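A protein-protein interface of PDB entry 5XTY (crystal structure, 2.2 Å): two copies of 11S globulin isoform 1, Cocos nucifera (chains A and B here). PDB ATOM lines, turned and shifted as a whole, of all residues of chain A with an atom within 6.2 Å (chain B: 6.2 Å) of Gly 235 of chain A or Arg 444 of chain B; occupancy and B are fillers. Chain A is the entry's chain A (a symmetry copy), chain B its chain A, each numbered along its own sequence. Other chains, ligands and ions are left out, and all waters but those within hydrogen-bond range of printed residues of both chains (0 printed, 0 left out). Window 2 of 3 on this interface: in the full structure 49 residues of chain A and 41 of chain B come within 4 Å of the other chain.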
ATOM      1  N   LEU A 230      -3.197  -7.550 -31.757  1.00  0.00           N
ATOM      2  CA  LEU A 230      -4.094  -8.381 -30.971  1.00  0.00           C
ATOM      3  C   LEU A 230      -3.759  -8.310 -29.491  1.00  0.00           C
ATOM      4  O   LEU A 230      -4.588  -7.912 -28.672  1.00  0.00           O
ATOM      5  CB  LEU A 230      -4.005  -9.818 -31.480  1.00  0.00           C
ATOM      6  CG  LEU A 230      -5.290 -10.627 -31.562  1.00  0.00           C
ATOM      7  CD1 LEU A 230      -6.436  -9.712 -31.891  1.00  0.00           C
ATOM      8  CD2 LEU A 230      -5.150 -11.683 -32.640  1.00  0.00           C
ATOM      9  N   ALA A 231      -2.535  -8.688 -29.135  1.00  0.00           N
ATOM     10  CA  ALA A 231      -2.102  -8.555 -27.752  1.00  0.00           C
ATOM     11  C   ALA A 231      -2.363  -7.145 -27.261  1.00  0.00           C
ATOM     12  O   ALA A 231      -3.132  -6.938 -26.317  1.00  0.00           O
ATOM     13  CB  ALA A 231      -0.623  -8.914 -27.614  1.00  0.00           C
ATOM     14  N   ALA A 232      -1.766  -6.154 -27.930  1.00  0.00           N
ATOM     15  CA  ALA A 232      -2.047  -4.773 -27.565  1.00  0.00           C
ATOM     16  C   ALA A 232      -3.533  -4.491 -27.636  1.00  0.00           C
ATOM     17  O   ALA A 232      -4.057  -3.719 -26.826  1.00  0.00           O
ATOM     18  CB  ALA A 232      -1.288  -3.803 -28.466  1.00  0.00           C
ATOM     19  N   ALA A 233      -4.233  -5.131 -28.572  1.00  0.00           N
ATOM     20  CA  ALA A 233      -5.668  -4.904 -28.683  1.00  0.00           C
ATOM     21  C   ALA A 233      -6.399  -5.370 -27.435  1.00  0.00           C
ATOM     22  O   ALA A 233      -7.335  -4.710 -26.974  1.00  0.00           O
ATOM     23  CB  ALA A 233      -6.224  -5.604 -29.916  1.00  0.00           C
ATOM     24  N   PHE A 234      -5.977  -6.493 -26.861  1.00  0.00           N
ATOM     25  CA  PHE A 234      -6.731  -7.089 -25.770  1.00  0.00           C
ATOM     26  C   PHE A 234      -6.082  -6.955 -24.403  1.00  0.00           C
ATOM     27  O   PHE A 234      -6.771  -7.143 -23.393  1.00  0.00           O
ATOM     28  CB  PHE A 234      -6.989  -8.572 -26.059  1.00  0.00           C
ATOM     29  CG  PHE A 234      -8.199  -8.812 -26.912  1.00  0.00           C
ATOM     30  CD1 PHE A 234      -8.074  -9.004 -28.277  1.00  0.00           C
ATOM     31  CD2 PHE A 234      -9.467  -8.826 -26.351  1.00  0.00           C
ATOM     32  CE1 PHE A 234      -9.189  -9.217 -29.067  1.00  0.00           C
ATOM     33  CE2 PHE A 234     -10.587  -9.035 -27.136  1.00  0.00           C
ATOM     34  CZ  PHE A 234     -10.445  -9.231 -28.497  1.00  0.00           C
ATOM     35  N   GLY A 235      -4.796  -6.628 -24.338  1.00  0.00           N
ATOM     36  CA  GLY A 235      -4.155  -6.552 -23.045  1.00  0.00           C
ATOM     37  C   GLY A 235      -3.917  -7.892 -22.404  1.00  0.00           C
ATOM     38  O   GLY A 235      -3.686  -7.967 -21.194  1.00  0.00           O
ATOM     39  N   VAL A 236      -3.997  -8.954 -23.170  1.00  0.00           N
ATOM     40  CA  VAL A 236      -3.569 -10.253 -22.699  1.00  0.00           C
ATOM     41  C   VAL A 236      -2.133 -10.452 -23.146  1.00  0.00           C
ATOM     42  O   VAL A 236      -1.668  -9.855 -24.121  1.00  0.00           O
ATOM     43  CB  VAL A 236      -4.473 -11.385 -23.219  1.00  0.00           C
ATOM     44  CG1 VAL A 236      -4.216 -11.611 -24.686  1.00  0.00           C
ATOM     45  CG2 VAL A 236      -4.244 -12.680 -22.436  1.00  0.00           C
ATOM     46  N   ASN A 237      -1.422 -11.299 -22.421  1.00  0.00           N
ATOM     47  CA  ASN A 237      -0.075 -11.654 -22.814  1.00  0.00           C
ATOM     48  C   ASN A 237      -0.050 -12.120 -24.259  1.00  0.00           C
ATOM     49  O   ASN A 237      -1.023 -12.663 -24.780  1.00  0.00           O
ATOM     50  CB  ASN A 237       0.470 -12.754 -21.915  1.00  0.00           C
ATOM     51  CG  ASN A 237      -0.204 -14.069 -22.160  1.00  0.00           C
ATOM     52  OD1 ASN A 237       0.285 -14.896 -22.919  1.00  0.00           O
ATOM     53  ND2 ASN A 237      -1.340 -14.273 -21.515  1.00  0.00           N
ATOM     54  N   ARG B 439     -10.165 -21.265 -17.057  1.00  0.00           N
ATOM     55  CA  ARG B 439     -11.070 -20.186 -16.700  1.00  0.00           C
ATOM     56  C   ARG B 439     -10.341 -18.852 -16.648  1.00  0.00           C
ATOM     57  O   ARG B 439     -10.785 -17.864 -17.244  1.00  0.00           O
ATOM     58  CB  ARG B 439     -11.734 -20.491 -15.359  1.00  0.00           C
ATOM     59  CG  ARG B 439     -13.018 -19.727 -15.124  1.00  0.00           C
ATOM     60  CD  ARG B 439     -13.029 -19.007 -13.797  1.00  0.00           C
ATOM     61  NE  ARG B 439     -12.059 -17.920 -13.753  1.00  0.00           N
ATOM     62  CZ  ARG B 439     -12.222 -16.739 -14.335  1.00  0.00           C
ATOM     63  NH1 ARG B 439     -13.319 -16.473 -15.024  1.00  0.00           N
ATOM     64  NH2 ARG B 439     -11.280 -15.824 -14.223  1.00  0.00           N
ATOM     65  N   ASP B 440      -9.195 -18.814 -15.961  1.00  0.00           N
ATOM     66  CA  ASP B 440      -8.540 -17.532 -15.737  1.00  0.00           C
ATOM     67  C   ASP B 440      -8.146 -16.892 -17.050  1.00  0.00           C
ATOM     68  O   ASP B 440      -8.147 -15.667 -17.164  1.00  0.00           O
ATOM     69  CB  ASP B 440      -7.335 -17.688 -14.808  1.00  0.00           C
ATOM     70  CG  ASP B 440      -6.084 -18.101 -15.532  1.00  0.00           C
ATOM     71  OD1 ASP B 440      -6.190 -18.798 -16.559  1.00  0.00           O
ATOM     72  OD2 ASP B 440      -4.987 -17.723 -15.066  1.00  0.00           O
ATOM     73  N   GLU B 441      -7.838 -17.694 -18.062  1.00  0.00           N
ATOM     74  CA  GLU B 441      -7.722 -17.118 -19.391  1.00  0.00           C
ATOM     75  C   GLU B 441      -9.051 -16.533 -19.832  1.00  0.00           C
ATOM     76  O   GLU B 441      -9.126 -15.373 -20.250  1.00  0.00           O
ATOM     77  CB  GLU B 441      -7.252 -18.162 -20.389  1.00  0.00           C
ATOM     78  CG  GLU B 441      -5.886 -18.689 -20.125  1.00  0.00           C
ATOM     79  CD  GLU B 441      -5.940 -20.123 -19.733  1.00  0.00           C
ATOM     80  OE1 GLU B 441      -6.307 -20.388 -18.581  1.00  0.00           O
ATOM     81  OE2 GLU B 441      -5.639 -20.986 -20.577  1.00  0.00           O
ATOM     82  N   ALA B 442     -10.115 -17.329 -19.732  1.00  0.00           N
ATOM     83  CA  ALA B 442     -11.417 -16.891 -20.203  1.00  0.00           C
ATOM     84  C   ALA B 442     -11.698 -15.479 -19.742  1.00  0.00           C
ATOM     85  O   ALA B 442     -11.897 -14.570 -20.549  1.00  0.00           O
ATOM     86  CB  ALA B 442     -12.504 -17.839 -19.703  1.00  0.00           C
ATOM     87  N   ARG B 443     -11.655 -15.262 -18.442  1.00  0.00           N
ATOM     88  CA  ARG B 443     -12.015 -13.947 -17.951  1.00  0.00           C
ATOM     89  C   ARG B 443     -11.012 -12.892 -18.382  1.00  0.00           C
ATOM     90  O   ARG B 443     -11.379 -11.721 -18.509  1.00  0.00           O
ATOM     91  CB  ARG B 443     -12.138 -13.982 -16.444  1.00  0.00           C
ATOM     92  CG  ARG B 443     -12.529 -12.692 -15.827  1.00  0.00           C
ATOM     93  CD  ARG B 443     -12.653 -12.871 -14.342  1.00  0.00           C
ATOM     94  NE  ARG B 443     -14.000 -12.571 -13.880  1.00  0.00           N
ATOM     95  CZ  ARG B 443     -14.443 -11.343 -13.648  1.00  0.00           C
ATOM     96  NH1 ARG B 443     -13.637 -10.309 -13.837  1.00  0.00           N
ATOM     97  NH2 ARG B 443     -15.687 -11.148 -13.226  1.00  0.00           N
ATOM     98  N   ARG B 444      -9.754 -13.275 -18.628  1.00  0.00           N
ATOM     99  CA  ARG B 444      -8.767 -12.277 -19.032  1.00  0.00           C
ATOM    100  C   ARG B 444      -9.188 -11.594 -20.316  1.00  0.00           C
ATOM    101  O   ARG B 444      -8.894 -10.411 -20.522  1.00  0.00           O
ATOM    102  CB  ARG B 444      -7.382 -12.905 -19.202  1.00  0.00           C
ATOM    103  CG  ARG B 444      -6.220 -11.990 -18.757  1.00  0.00           C
ATOM    104  CD  ARG B 444      -5.917 -10.882 -19.773  1.00  0.00           C
ATOM    105  NE  ARG B 444      -4.893  -9.948 -19.314  1.00  0.00           N
ATOM    106  CZ  ARG B 444      -5.157  -8.829 -18.650  1.00  0.00           C
ATOM    107  NH1 ARG B 444      -6.409  -8.500 -18.367  1.00  0.00           N
ATOM    108  NH2 ARG B 444      -4.171  -8.039 -18.270  1.00  0.00           N
ATOM    109  N   VAL B 445      -9.896 -12.318 -21.175  1.00  0.00           N
ATOM    110  CA  VAL B 445     -10.463 -11.712 -22.370  1.00  0.00           C
ATOM    111  C   VAL B 445     -11.785 -11.026 -22.058  1.00  0.00           C
ATOM    112  O   VAL B 445     -12.090  -9.963 -22.605  1.00  0.00           O
ATOM    113  CB  VAL B 445     -10.627 -12.782 -23.454  1.00  0.00           C
ATOM    114  CG1 VAL B 445     -11.147 -12.154 -24.718  1.00  0.00           C
ATOM    115  CG2 VAL B 445      -9.307 -13.486 -23.689  1.00  0.00           C
ATOM    116  N   LYS B 446     -12.598 -11.619 -21.192  1.00  0.00           N
ATOM    117  CA  LYS B 446     -13.861 -11.013 -20.826  1.00  0.00           C
ATOM    118  C   LYS B 446     -13.669 -10.116 -19.616  1.00  0.00           C
ATOM    119  O   LYS B 446     -13.779 -10.565 -18.480  1.00  0.00           O
ATOM    120  CB  LYS B 446     -14.895 -12.074 -20.548  1.00  0.00           C
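Ala 231 of chain A touches none of the printed residues of chain B. Printed residues of chain B within 4 Å of Phe 234 of chain A: Val 445. Gly 235 of chain A touches just one residue of chain B: Arg 444 (3.0 Å). Of the printed residues of chain B, Val 236 of chain A touches Arg 444. Arg 443 of chain B touches none of the printed residues of chain A. Printed residues of chain A within 4 Å of Arg 444 of chain B: Gly 235 (3.0 Å) and Val 236 (3.6 Å). Of the printed residues of chain A, Val 445 of chain B touches Phe 234. The nearest printed residue of chain A that does not touch Arg 444 of chain B is Phe 234 of chain A (4.8 Å).
O of Gly 235 of chain A lies within hydrogen-bond range of NH2 of Arg 444 of chain B, at 3.0 Å.
No position is printed for both chains. Of the 3 pairs that touch across the chains among the printed residues, none has its exchanged pair printed and touching as well.
Printed residues of chain B that touch a printed residue of chain A: Arg 444 and Val 445. Printed residues of chain A that touch a printed residue of chain B: Phe 234, Gly 235 and Val 236. Along chain A the printed residues that touch a printed residue of chain B span positions 234 to 236. Among the printed residues, 3 pairs touch across the chains. Among the printed residues, no Asp or Glu carboxylate lies within 4 Å of a Lys or Arg side-chain nitrogen of the other chain.
Among the printed residues, merely in contact across the chains: Val 236 of chain A with Arg 444 of chain B (3.6 Å) and Phe 234 of chain A with Val 445 of chain B (3.99 Å).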
